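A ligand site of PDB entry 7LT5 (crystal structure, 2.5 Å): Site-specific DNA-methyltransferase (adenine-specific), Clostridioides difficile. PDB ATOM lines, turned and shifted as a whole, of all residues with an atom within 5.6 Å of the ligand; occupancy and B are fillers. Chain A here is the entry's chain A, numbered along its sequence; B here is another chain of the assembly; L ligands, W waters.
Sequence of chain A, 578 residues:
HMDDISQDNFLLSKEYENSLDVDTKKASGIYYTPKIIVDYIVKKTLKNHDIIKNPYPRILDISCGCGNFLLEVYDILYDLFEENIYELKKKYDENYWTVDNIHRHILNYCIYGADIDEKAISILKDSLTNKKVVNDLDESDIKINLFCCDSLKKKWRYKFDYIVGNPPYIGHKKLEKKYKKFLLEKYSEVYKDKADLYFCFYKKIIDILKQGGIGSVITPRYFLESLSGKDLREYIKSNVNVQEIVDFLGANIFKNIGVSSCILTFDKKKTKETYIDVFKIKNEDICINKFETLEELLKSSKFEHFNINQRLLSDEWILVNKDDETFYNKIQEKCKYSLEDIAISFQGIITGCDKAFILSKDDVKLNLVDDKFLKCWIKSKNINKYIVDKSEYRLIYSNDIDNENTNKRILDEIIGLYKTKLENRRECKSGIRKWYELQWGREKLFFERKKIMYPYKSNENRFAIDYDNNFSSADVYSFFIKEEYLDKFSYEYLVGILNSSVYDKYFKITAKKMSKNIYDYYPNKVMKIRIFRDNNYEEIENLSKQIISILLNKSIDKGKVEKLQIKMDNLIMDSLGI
An oxygen (O5) of the ligand is in hydrogen-bond range of the side-chain carboxylate of Asp 115 (2.6 Å).
S1 of the ligand sits close to N of Tyr 31, 3.6 Å away.
The side-chain carboxylate of Asp 61 is in salt-bridge range of a nitrogen (N1) of the ligand, at 3.3 Å.
The backbone NH (N) of Thr 33 sits at hydrogen-bond distance from an oxygen (O2) of the ligand (3.0 Å).
O1 of the ligand lies within hydrogen-bond range of OG1 of Thr 33 (2.5 Å).
O of Ser 63 is in hydrogen-bond range of N1 of the ligand (2.7 Å).
A nitrogen (N4) of the ligand sits at hydrogen-bond distance from the side-chain carboxylate (OD1) of Asp 150 (2.8 Å).
An oxygen (O2) of the ligand lies close to the side-chain amide nitrogen (ND2) of Asn 68 (3.4 Å).
N5 of the ligand is in hydrogen-bond range of N of Ser 151.
Water W1 lies within hydrogen-bond range of O2 of the ligand (3.0 Å), N of Asn 68 (3.0 Å), O of Cys 64 (3.3 Å) and N of Cys 66 (3.3 Å).
N of Asp 117 is in hydrogen-bond range of OD1 of Asp 115 (2.7 Å).
O of Asp 115 lies within hydrogen-bond range of N of Cys 149 (3.1 Å).
The side-chain amide nitrogen (ND2) of Asn 166 lies within hydrogen-bond range of N1 of DA 8 of chain B, at 2.9 Å.
The backbone NH of Ala 114 sits at hydrogen-bond distance from the backbone carbonyl oxygen of Asp 61, at 2.9 Å.
N of Ser 63 is in hydrogen-bond range of O of Ala 114.
OH of Tyr 32 lies within hydrogen-bond range of N of Cys 66, at 3.4 Å.
The backbone carbonyl oxygen (O) of Ile 62 sits at hydrogen-bond distance from the side-chain hydroxyl (OG) of Ser 151 (2.8 Å).
The side-chain carboxylate of Asp 115 lies within hydrogen-bond range of the backbone NH of Gly 65 (2.9 Å).
The backbone carbonyl oxygen (O) of Gly 29 lies close to a sulfur (S1) of the ligand, at 3.4 Å.
Merely in contact with the ligand: Ser 28 (3.4 Å), Ile 30 (3.9 Å), Tyr 32 (3.3 Å), Ile 62 (3.5 Å), Cys 64 (3.4 Å), Gly 65 (3.8 Å), Phe 69 (3.2 Å), Ile 116 (3.5 Å), Asp 117 (3.8 Å), Cys 149 (3.6 Å), Asn 166 (3.2 Å), Pro 168 (3.4 Å), Tyr 179 (3.8 Å), Phe 201 (3.6 Å) and DA 8 of chain B (3.9 Å).
The nearest printed residue that does not touch the ligand is Pro 167 (4.3 Å).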
ATOM      1  N   SER A  28     -13.926 -19.650  24.903  1.00  0.00           N
ATOM      2  CA  SER A  28     -13.931 -20.951  24.260  1.00  0.00           C
ATOM      3  C   SER A  28     -13.409 -20.923  22.827  1.00  0.00           C
ATOM      4  O   SER A  28     -13.422 -21.966  22.158  1.00  0.00           O
ATOM      5  CB  SER A  28     -15.339 -21.561  24.289  1.00  0.00           C
ATOM      6  OG  SER A  28     -15.770 -21.787  25.613  1.00  0.00           O
ATOM      7  N   GLY A  29     -12.957 -19.774  22.345  1.00  0.00           N
ATOM      8  CA  GLY A  29     -12.443 -19.680  20.983  1.00  0.00           C
ATOM      9  C   GLY A  29     -13.480 -19.995  19.928  1.00  0.00           C
ATOM     10  O   GLY A  29     -13.191 -20.729  18.969  1.00  0.00           O
ATOM     11  N   ILE A  30     -14.688 -19.448  20.072  1.00  0.00           N
ATOM     12  CA  ILE A  30     -15.802 -19.746  19.161  1.00  0.00           C
ATOM     13  C   ILE A  30     -15.735 -18.724  18.031  1.00  0.00           C
ATOM     14  O   ILE A  30     -16.367 -17.669  18.073  1.00  0.00           O
ATOM     15  CB  ILE A  30     -17.150 -19.738  19.878  1.00  0.00           C
ATOM     16  CG1 ILE A  30     -17.075 -20.614  21.137  1.00  0.00           C
ATOM     17  CG2 ILE A  30     -18.242 -20.234  18.953  1.00  0.00           C
ATOM     18  CD1 ILE A  30     -18.335 -20.583  21.976  1.00  0.00           C
ATOM     19  N   TYR A  31     -14.950 -19.052  17.001  1.00  0.00           N
ATOM     20  CA  TYR A  31     -14.810 -18.206  15.809  1.00  0.00           C
ATOM     21  C   TYR A  31     -14.794 -19.128  14.588  1.00  0.00           C
ATOM     22  O   TYR A  31     -13.778 -19.769  14.310  1.00  0.00           O
ATOM     23  CB  TYR A  31     -13.550 -17.353  15.886  1.00  0.00           C
ATOM     24  CG  TYR A  31     -13.470 -16.482  17.118  1.00  0.00           C
ATOM     25  CD1 TYR A  31     -14.045 -15.219  17.139  1.00  0.00           C
ATOM     26  CD2 TYR A  31     -12.810 -16.925  18.264  1.00  0.00           C
ATOM     27  CE1 TYR A  31     -13.969 -14.421  18.272  1.00  0.00           C
ATOM     28  CE2 TYR A  31     -12.735 -16.131  19.388  1.00  0.00           C
ATOM     29  CZ  TYR A  31     -13.317 -14.884  19.394  1.00  0.00           C
ATOM     30  OH  TYR A  31     -13.238 -14.087  20.506  1.00  0.00           O
ATOM     31  N   TYR A  32     -15.904 -19.180  13.866  1.00  0.00           N
ATOM     32  CA  TYR A  32     -16.062 -20.140  12.791  1.00  0.00           C
ATOM     33  C   TYR A  32     -15.346 -19.687  11.522  1.00  0.00           C
ATOM     34  O   TYR A  32     -15.168 -18.483  11.277  1.00  0.00           O
ATOM     35  CB  TYR A  32     -17.544 -20.386  12.503  1.00  0.00           C
ATOM     36  CG  TYR A  32     -18.304 -21.016  13.646  1.00  0.00           C
ATOM     37  CD1 TYR A  32     -17.631 -21.627  14.700  1.00  0.00           C
ATOM     38  CD2 TYR A  32     -19.695 -21.014  13.677  1.00  0.00           C
ATOM     39  CE1 TYR A  32     -18.319 -22.205  15.757  1.00  0.00           C
ATOM     40  CE2 TYR A  32     -20.391 -21.588  14.733  1.00  0.00           C
ATOM     41  CZ  TYR A  32     -19.689 -22.192  15.759  1.00  0.00           C
ATOM     42  OH  TYR A  32     -20.377 -22.774  16.807  1.00  0.00           O
ATOM     43  N   THR A  33     -14.935 -20.670  10.714  1.00  0.00           N
ATOM     44  CA  THR A  33     -14.099 -20.486   9.529  1.00  0.00           C
ATOM     45  C   THR A  33     -14.956 -20.043   8.329  1.00  0.00           C
ATOM     46  O   THR A  33     -16.049 -20.567   8.120  1.00  0.00           O
ATOM     47  CB  THR A  33     -13.386 -21.799   9.197  1.00  0.00           C
ATOM     48  OG1 THR A  33     -12.609 -22.216  10.330  1.00  0.00           O
ATOM     49  CG2 THR A  33     -12.457 -21.633   8.010  1.00  0.00           C
ATOM     50  N   VAL A  38     -12.816 -23.219   4.146  1.00  0.00           N
ATOM     51  CA  VAL A  38     -13.430 -24.534   4.313  1.00  0.00           C
ATOM     52  C   VAL A  38     -13.420 -25.300   2.991  1.00  0.00           C
ATOM     53  O   VAL A  38     -13.080 -26.475   2.947  1.00  0.00           O
ATOM     54  CB  VAL A  38     -14.868 -24.390   4.869  1.00  0.00           C
ATOM     55  CG1 VAL A  38     -15.560 -25.741   4.873  1.00  0.00           C
ATOM     56  CG2 VAL A  38     -14.837 -23.790   6.260  1.00  0.00           C
ATOM     57  N   ASP A  61     -13.947 -33.822  12.738  1.00  0.00           N
ATOM     58  CA  ASP A  61     -13.653 -32.470  13.195  1.00  0.00           C
ATOM     59  C   ASP A  61     -13.837 -32.442  14.708  1.00  0.00           C
ATOM     60  O   ASP A  61     -14.966 -32.505  15.191  1.00  0.00           O
ATOM     61  CB  ASP A  61     -14.548 -31.440  12.507  1.00  0.00           C
ATOM     62  CG  ASP A  61     -14.156 -30.000  12.827  1.00  0.00           C
ATOM     63  OD1 ASP A  61     -13.273 -29.786  13.679  1.00  0.00           O
ATOM     64  OD2 ASP A  61     -14.758 -29.083  12.234  1.00  0.00           O
ATOM     65  N   ILE A  62     -12.731 -32.348  15.457  1.00  0.00           N
ATOM     66  CA  ILE A  62     -12.805 -32.359  16.922  1.00  0.00           C
ATOM     67  C   ILE A  62     -13.240 -31.023  17.499  1.00  0.00           C
ATOM     68  O   ILE A  62     -13.379 -30.911  18.729  1.00  0.00           O
ATOM     69  CB  ILE A  62     -11.475 -32.742  17.593  1.00  0.00           C
ATOM     70  CG1 ILE A  62     -10.327 -31.882  17.053  1.00  0.00           C
ATOM     71  CG2 ILE A  62     -11.170 -34.209  17.407  1.00  0.00           C
ATOM     72  CD1 ILE A  62      -9.034 -32.131  17.769  1.00  0.00           C
ATOM     73  N   SER A  63     -13.432 -30.009  16.675  1.00  0.00           N
ATOM     74  CA  SER A  63     -13.945 -28.708  17.090  1.00  0.00           C
ATOM     75  C   SER A  63     -15.011 -28.240  16.120  1.00  0.00           C
ATOM     76  O   SER A  63     -15.001 -27.107  15.639  1.00  0.00           O
ATOM     77  CB  SER A  63     -12.815 -27.687  17.195  1.00  0.00           C
ATOM     78  OG  SER A  63     -11.831 -28.105  18.118  1.00  0.00           O
ATOM     79  N   CYS A  64     -15.968 -29.128  15.828  1.00  0.00           N
ATOM     80  CA  CYS A  64     -16.865 -28.916  14.700  1.00  0.00           C
ATOM     81  C   CYS A  64     -17.731 -27.675  14.861  1.00  0.00           C
ATOM     82  O   CYS A  64     -18.101 -27.038  13.862  1.00  0.00           O
ATOM     83  CB  CYS A  64     -17.751 -30.145  14.496  1.00  0.00           C
ATOM     84  SG  CYS A  64     -18.775 -30.562  15.925  1.00  0.00           S
ATOM     85  N   GLY A  65     -18.056 -27.290  16.090  1.00  0.00           N
ATOM     86  CA  GLY A  65     -18.953 -26.166  16.284  1.00  0.00           C
ATOM     87  C   GLY A  65     -20.315 -26.468  15.700  1.00  0.00           C
ATOM     88  O   GLY A  65     -20.902 -27.523  15.935  1.00  0.00           O
ATOM     89  N   CYS A  66     -20.834 -25.527  14.900  1.00  0.00           N
ATOM     90  CA  CYS A  66     -22.100 -25.738  14.210  1.00  0.00           C
ATOM     91  C   CYS A  66     -21.946 -26.546  12.924  1.00  0.00           C
ATOM     92  O   CYS A  66     -22.954 -26.916  12.319  1.00  0.00           O
ATOM     93  CB  CYS A  66     -22.769 -24.407  13.903  1.00  0.00           C
ATOM     94  SG  CYS A  66     -23.579 -23.627  15.317  1.00  0.00           S
ATOM     95  N   ASN A  68     -19.342 -25.959  10.123  1.00  0.00           N
ATOM     96  CA  ASN A  68     -18.894 -25.312   8.897  1.00  0.00           C
ATOM     97  C   ASN A  68     -18.110 -26.274   8.017  1.00  0.00           C
ATOM     98  O   ASN A  68     -18.212 -26.219   6.784  1.00  0.00           O
ATOM     99  CB  ASN A  68     -18.042 -24.077   9.224  1.00  0.00           C
ATOM    100  CG  ASN A  68     -18.878 -22.867   9.560  1.00  0.00           C
ATOM    101  OD1 ASN A  68     -20.076 -22.971   9.782  1.00  0.00           O
ATOM    102  ND2 ASN A  68     -18.234 -21.705   9.601  1.00  0.00           N
ATOM    103  N   PHE A  69     -17.319 -27.155   8.628  1.00  0.00           N
ATOM    104  CA  PHE A  69     -16.578 -28.130   7.846  1.00  0.00           C
ATOM    105  C   PHE A  69     -17.419 -29.366   7.530  1.00  0.00           C
ATOM    106  O   PHE A  69     -17.360 -29.885   6.401  1.00  0.00           O
ATOM    107  CB  PHE A  69     -15.311 -28.550   8.596  1.00  0.00           C
ATOM    108  CG  PHE A  69     -14.192 -27.557   8.484  1.00  0.00           C
ATOM    109  CD1 PHE A  69     -14.073 -26.517   9.395  1.00  0.00           C
ATOM    110  CD2 PHE A  69     -13.247 -27.666   7.472  1.00  0.00           C
ATOM    111  CE1 PHE A  69     -13.044 -25.605   9.295  1.00  0.00           C
ATOM    112  CE2 PHE A  69     -12.204 -26.751   7.369  1.00  0.00           C
ATOM    113  CZ  PHE A  69     -12.104 -25.722   8.287  1.00  0.00           C
ATOM    114  N   ALA A 114     -16.866 -33.387  17.208  1.00  0.00           N
ATOM    115  CA  ALA A 114     -16.751 -33.218  18.649  1.00  0.00           C
ATOM    116  C   ALA A 114     -16.707 -31.744  18.980  1.00  0.00           C
ATOM    117  O   ALA A 114     -16.142 -30.937  18.231  1.00  0.00           O
ATOM    118  CB  ALA A 114     -15.505 -33.918  19.195  1.00  0.00           C
ATOM    119  N   ASP A 115     -17.314 -31.378  20.116  1.00  0.00           N
ATOM    120  CA  ASP A 115     -17.292 -30.000  20.581  1.00  0.00           C
ATOM    121  C   ASP A 115     -17.861 -29.948  21.994  1.00  0.00           C
ATOM    122  O   ASP A 115     -18.759 -30.725  22.338  1.00  0.00           O
ATOM    123  CB  ASP A 115     -18.100 -29.074  19.666  1.00  0.00           C
ATOM    124  CG  ASP A 115     -17.733 -27.608  19.834  1.00  0.00           C
ATOM    125  OD1 ASP A 115     -17.819 -27.095  20.968  1.00  0.00           O
ATOM    126  OD2 ASP A 115     -17.326 -26.988  18.832  1.00  0.00           O
ATOM    127  N   ILE A 116     -17.332 -29.036  22.807  1.00  0.00           N
ATOM    128  CA  ILE A 116     -17.864 -28.822  24.156  1.00  0.00           C
ATOM    129  C   ILE A 116     -19.163 -28.028  24.156  1.00  0.00           C
ATOM    130  O   ILE A 116     -19.844 -27.997  25.196  1.00  0.00           O
ATOM    131  CB  ILE A 116     -16.862 -28.071  25.054  1.00  0.00           C
ATOM    132  CG1 ILE A 116     -16.541 -26.701  24.456  1.00  0.00           C
ATOM    133  CG2 ILE A 116     -15.594 -28.880  25.240  1.00  0.00           C
ATOM    134  CD1 ILE A 116     -15.679 -25.831  25.350  1.00  0.00           C
ATOM    135  N   ASP A 117     -19.525 -27.404  23.040  1.00  0.00           N
ATOM    136  CA  ASP A 117     -20.700 -26.544  22.965  1.00  0.00           C
ATOM    137  C   ASP A 117     -21.918 -27.396  22.640  1.00  0.00           C
ATOM    138  O   ASP A 117     -22.060 -27.907  21.519  1.00  0.00           O
ATOM    139  CB  ASP A 117     -20.484 -25.458  21.910  1.00  0.00           C
ATOM    140  CG  ASP A 117     -21.544 -24.376  21.954  1.00  0.00           C
ATOM    141  OD1 ASP A 117     -22.541 -24.538  22.696  1.00  0.00           O
ATOM    142  OD2 ASP A 117     -21.377 -23.364  21.246  1.00  0.00           O
ATOM    143  N   ALA A 120     -24.335 -25.791  19.888  1.00  0.00           N
ATOM    144  CA  ALA A 120     -23.755 -25.910  18.557  1.00  0.00           C
ATOM    145  C   ALA A 120     -23.851 -27.352  18.052  1.00  0.00           C
ATOM    146  O   ALA A 120     -24.117 -27.594  16.869  1.00  0.00           O
ATOM    147  CB  ALA A 120     -22.304 -25.446  18.565  1.00  0.00           C
ATOM    148  N   CYS A 149     -18.172 -33.163  24.189  1.00  0.00           N
ATOM    149  CA  CYS A 149     -17.105 -33.554  25.113  1.00  0.00           C
ATOM    150  C   CYS A 149     -15.923 -32.610  24.928  1.00  0.00           C
ATOM    151  O   CYS A 149     -15.849 -31.834  23.971  1.00  0.00           O
ATOM    152  CB  CYS A 149     -16.664 -34.997  24.857  1.00  0.00           C
ATOM    153  SG  CYS A 149     -15.814 -35.223  23.281  1.00  0.00           S
ATOM    154  N   ASP A 150     -14.992 -32.693  25.873  1.00  0.00           N
ATOM    155  CA  ASP A 150     -13.685 -32.060  25.746  1.00  0.00           C
ATOM    156  C   ASP A 150     -12.805 -33.000  24.922  1.00  0.00           C
ATOM    157  O   ASP A 150     -12.435 -34.082  25.394  1.00  0.00           O
ATOM    158  CB  ASP A 150     -13.088 -31.791  27.122  1.00  0.00           C
ATOM    159  CG  ASP A 150     -11.833 -30.938  27.067  1.00  0.00           C
ATOM    160  OD1 ASP A 150     -11.070 -31.019  26.074  1.00  0.00           O
ATOM    161  OD2 ASP A 150     -11.593 -30.171  28.031  1.00  0.00           O
ATOM    162  N   SER A 151     -12.456 -32.580  23.708  1.00  0.00           N
ATOM    163  CA  SER A 151     -11.675 -33.444  22.818  1.00  0.00           C
ATOM    164  C   SER A 151     -10.308 -33.776  23.408  1.00  0.00           C
ATOM    165  O   SER A 151      -9.735 -34.814  23.079  1.00  0.00           O
ATOM    166  CB  SER A 151     -11.516 -32.775  21.449  1.00  0.00           C
ATOM    167  OG  SER A 151     -12.764 -32.668  20.780  1.00  0.00           O
ATOM    168  N   LEU A 152      -9.786 -32.909  24.274  1.00  0.00           N
ATOM    169  CA  LEU A 152      -8.493 -33.158  24.891  1.00  0.00           C
ATOM    170  C   LEU A 152      -8.572 -34.106  26.078  1.00  0.00           C
ATOM    171  O   LEU A 152      -7.521 -34.540  26.572  1.00  0.00           O
ATOM    172  CB  LEU A 152      -7.848 -31.837  25.323  1.00  0.00           C
ATOM    173  CG  LEU A 152      -7.621 -30.837  24.185  1.00  0.00           C
ATOM    174  CD1 LEU A 152      -6.795 -29.654  24.680  1.00  0.00           C
ATOM    175  CD2 LEU A 152      -6.938 -31.502  22.997  1.00  0.00           C
ATOM    176  N   GLY A 165     -10.523 -29.098  10.323  1.00  0.00           N
ATOM    177  CA  GLY A 165     -11.234 -28.173  11.190  1.00  0.00           C
ATOM    178  C   GLY A 165     -10.344 -27.031  11.630  1.00  0.00           C
ATOM    179  O   GLY A 165      -9.267 -26.801  11.091  1.00  0.00           O
ATOM    180  N   ASN A 166     -10.831 -26.317  12.643  1.00  0.00           N
ATOM    181  CA  ASN A 166     -10.220 -25.116  13.198  1.00  0.00           C
ATOM    182  C   ASN A 166     -10.297 -25.184  14.720  1.00  0.00           C
ATOM    183  O   ASN A 166     -11.385 -25.066  15.283  1.00  0.00           O
ATOM    184  CB  ASN A 166     -10.927 -23.868  12.657  1.00  0.00           C
ATOM    185  CG  ASN A 166     -10.363 -22.583  13.224  1.00  0.00           C
ATOM    186  OD1 ASN A 166      -9.185 -22.506  13.599  1.00  0.00           O
ATOM    187  ND2 ASN A 166     -11.200 -21.564  13.304  1.00  0.00           N
ATOM    188  N   PRO A 167      -9.179 -25.386  15.401  1.00  0.00           N
ATOM    189  CA  PRO A 167      -9.205 -25.543  16.859  1.00  0.00           C
ATOM    190  C   PRO A 167      -9.405 -24.209  17.554  1.00  0.00           C
ATOM    191  O   PRO A 167      -9.236 -23.152  16.935  1.00  0.00           O
ATOM    192  CB  PRO A 167      -7.826 -26.133  17.177  1.00  0.00           C
ATOM    193  CG  PRO A 167      -6.942 -25.552  16.108  1.00  0.00           C
ATOM    194  CD  PRO A 167      -7.801 -25.444  14.869  1.00  0.00           C
ATOM    195  N   PRO A 168      -9.772 -24.214  18.839  1.00  0.00           N
ATOM    196  CA  PRO A 168      -9.802 -22.956  19.582  1.00  0.00           C
ATOM    197  C   PRO A 168      -8.395 -22.477  19.918  1.00  0.00           C
ATOM    198  O   PRO A 168      -7.501 -23.282  20.198  1.00  0.00           O
ATOM    199  CB  PRO A 168     -10.584 -23.320  20.851  1.00  0.00           C
ATOM    200  CG  PRO A 168     -10.306 -24.773  21.036  1.00  0.00           C
ATOM    201  CD  PRO A 168     -10.263 -25.341  19.645  1.00  0.00           C
ATOM    202  N   TYR A 179      -7.165 -26.102  34.535  1.00  0.00           N
ATOM    203  CA  TYR A 179      -7.072 -26.652  33.186  1.00  0.00           C
ATOM    204  C   TYR A 179      -5.643 -26.550  32.654  1.00  0.00           C
ATOM    205  O   TYR A 179      -5.160 -27.456  31.958  1.00  0.00           O
ATOM    206  CB  TYR A 179      -8.048 -25.940  32.252  1.00  0.00           C
ATOM    207  CG  TYR A 179      -8.349 -26.719  30.993  1.00  0.00           C
ATOM    208  CD1 TYR A 179      -7.521 -26.620  29.880  1.00  0.00           C
ATOM    209  CD2 TYR A 179      -9.447 -27.566  30.917  1.00  0.00           C
ATOM    210  CE1 TYR A 179      -7.782 -27.340  28.732  1.00  0.00           C
ATOM    211  CE2 TYR A 179      -9.725 -28.272  29.777  1.00  0.00           C
ATOM    212  CZ  TYR A 179      -8.882 -28.162  28.679  1.00  0.00           C
ATOM    213  OH  TYR A 179      -9.164 -28.877  27.542  1.00  0.00           O
ATOM    214  N   LEU A 197      -3.386 -23.406  23.549  1.00  0.00           N
ATOM    215  CA  LEU A 197      -4.213 -24.606  23.545  1.00  0.00           C
ATOM    216  C   LEU A 197      -4.180 -25.332  22.203  1.00  0.00           C
ATOM    217  O   LEU A 197      -4.250 -26.575  22.146  1.00  0.00           O
ATOM    218  CB  LEU A 197      -5.652 -24.228  23.910  1.00  0.00           C
ATOM    219  CG  LEU A 197      -6.706 -25.323  24.071  1.00  0.00           C
ATOM    220  CD1 LEU A 197      -6.456 -26.128  25.323  1.00  0.00           C
ATOM    221  CD2 LEU A 197      -8.098 -24.699  24.102  1.00  0.00           C
ATOM    222  N   PHE A 201      -4.242 -29.231  20.672  1.00  0.00           N
ATOM    223  CA  PHE A 201      -5.141 -29.710  19.631  1.00  0.00           C
ATOM    224  C   PHE A 201      -4.366 -30.308  18.459  1.00  0.00           C
ATOM    225  O   PHE A 201      -4.788 -31.324  17.889  1.00  0.00           O
ATOM    226  CB  PHE A 201      -6.080 -28.604  19.167  1.00  0.00           C
ATOM    227  CG  PHE A 201      -7.323 -28.500  19.995  1.00  0.00           C
ATOM    228  CD1 PHE A 201      -7.346 -27.754  21.162  1.00  0.00           C
ATOM    229  CD2 PHE A 201      -8.475 -29.176  19.619  1.00  0.00           C
ATOM    230  CE1 PHE A 201      -8.501 -27.673  21.924  1.00  0.00           C
ATOM    231  CE2 PHE A 201      -9.627 -29.091  20.367  1.00  0.00           C
ATOM    232  CZ  PHE A 201      -9.637 -28.341  21.531  1.00  0.00           C
ATOM    233  P    DA B   8      -4.518 -13.632  21.773  1.00  0.00           P
ATOM    234  OP1  DA B   8      -5.311 -12.714  22.631  1.00  0.00           O
ATOM    235  OP2  DA B   8      -4.225 -15.013  22.243  1.00  0.00           O
ATOM    236  O5'  DA B   8      -5.217 -13.740  20.348  1.00  0.00           O
ATOM    237  C5'  DA B   8      -6.154 -14.777  20.086  1.00  0.00           C
ATOM    238  C4'  DA B   8      -7.117 -14.360  18.985  1.00  0.00           C
ATOM    239  O4'  DA B   8      -7.527 -15.529  18.229  1.00  0.00           O
ATOM    240  C3'  DA B   8      -8.402 -13.685  19.466  1.00  0.00           C
ATOM    241  O3'  DA B   8      -8.727 -12.606  18.616  1.00  0.00           O
ATOM    242  C2'  DA B   8      -9.427 -14.811  19.351  1.00  0.00           C
ATOM    243  C1'  DA B   8      -8.931 -15.522  18.106  1.00  0.00           C
ATOM    244  N9   DA B   8      -9.396 -16.900  17.998  1.00  0.00           N
ATOM    245  C8   DA B   8      -9.524 -17.812  18.998  1.00  0.00           C
ATOM    246  N7   DA B   8      -9.959 -18.987  18.600  1.00  0.00           N
ATOM    247  C5   DA B   8     -10.125 -18.825  17.227  1.00  0.00           C
ATOM    248  C6   DA B   8     -10.556 -19.706  16.214  1.00  0.00           C
ATOM    249  N6   DA B   8     -10.923 -20.972  16.441  1.00  0.00           N
ATOM    250  N1   DA B   8     -10.598 -19.221  14.948  1.00  0.00           N
ATOM    251  C2   DA B   8     -10.230 -17.956  14.721  1.00  0.00           C
ATOM    252  N3   DA B   8      -9.799 -17.042  15.599  1.00  0.00           N
ATOM    253  C4   DA B   8      -9.779 -17.550  16.844  1.00  0.00           C
HETATM  254  N1  LIG L   1     -14.350 -25.942  13.249  1.00  0.00           N
HETATM  255  C1  LIG L   1     -15.427 -24.970  13.234  1.00  0.00           C
HETATM  256  C2  LIG L   1     -15.556 -24.291  14.596  1.00  0.00           C
HETATM  257  C3  LIG L   1     -14.309 -23.515  15.005  1.00  0.00           C
HETATM  258  S1  LIG L   1     -14.506 -22.626  16.524  1.00  0.00           S
HETATM  259  C4  LIG L   1     -15.175 -23.943  12.180  1.00  0.00           C
HETATM  260  O1  LIG L   1     -14.017 -23.820  11.723  1.00  0.00           O
HETATM  261  O2  LIG L   1     -16.147 -23.248  11.792  1.00  0.00           O
HETATM  262  C5  LIG L   1     -13.704 -23.679  17.683  1.00  0.00           C
HETATM  263  C6  LIG L   1     -14.661 -24.600  18.449  1.00  0.00           C
HETATM  264  O3  LIG L   1     -13.916 -25.412  19.342  1.00  0.00           O
HETATM  265  C7  LIG L   1     -15.679 -23.824  19.316  1.00  0.00           C
HETATM  266  O4  LIG L   1     -17.007 -24.063  18.821  1.00  0.00           O
HETATM  267  C8  LIG L   1     -15.525 -24.430  20.722  1.00  0.00           C
HETATM  268  O5  LIG L   1     -16.811 -24.758  21.251  1.00  0.00           O
HETATM  269  C9  LIG L   1     -14.773 -25.705  20.413  1.00  0.00           C
HETATM  270  N2  LIG L   1     -13.962 -26.137  21.581  1.00  0.00           N
HETATM  271  C10 LIG L   1     -13.349 -25.329  22.463  1.00  0.00           C
HETATM  272  N3  LIG L   1     -12.699 -26.077  23.394  1.00  0.00           N
HETATM  273  C11 LIG L   1     -12.928 -27.359  23.075  1.00  0.00           C
HETATM  274  C12 LIG L   1     -12.515 -28.654  23.679  1.00  0.00           C
HETATM  275  N4  LIG L   1     -11.733 -28.678  24.791  1.00  0.00           N
HETATM  276  N5  LIG L   1     -12.923 -29.798  23.099  1.00  0.00           N
HETATM  277  C13 LIG L   1     -13.680 -29.697  22.016  1.00  0.00           C
HETATM  278  N6  LIG L   1     -14.096 -28.603  21.413  1.00  0.00           N
HETATM  279  C14 LIG L   1     -13.731 -27.403  21.929  1.00  0.00           C
HETATM  280  O   HOH W   1     -18.922 -24.148  12.529  1.00  0.00           O
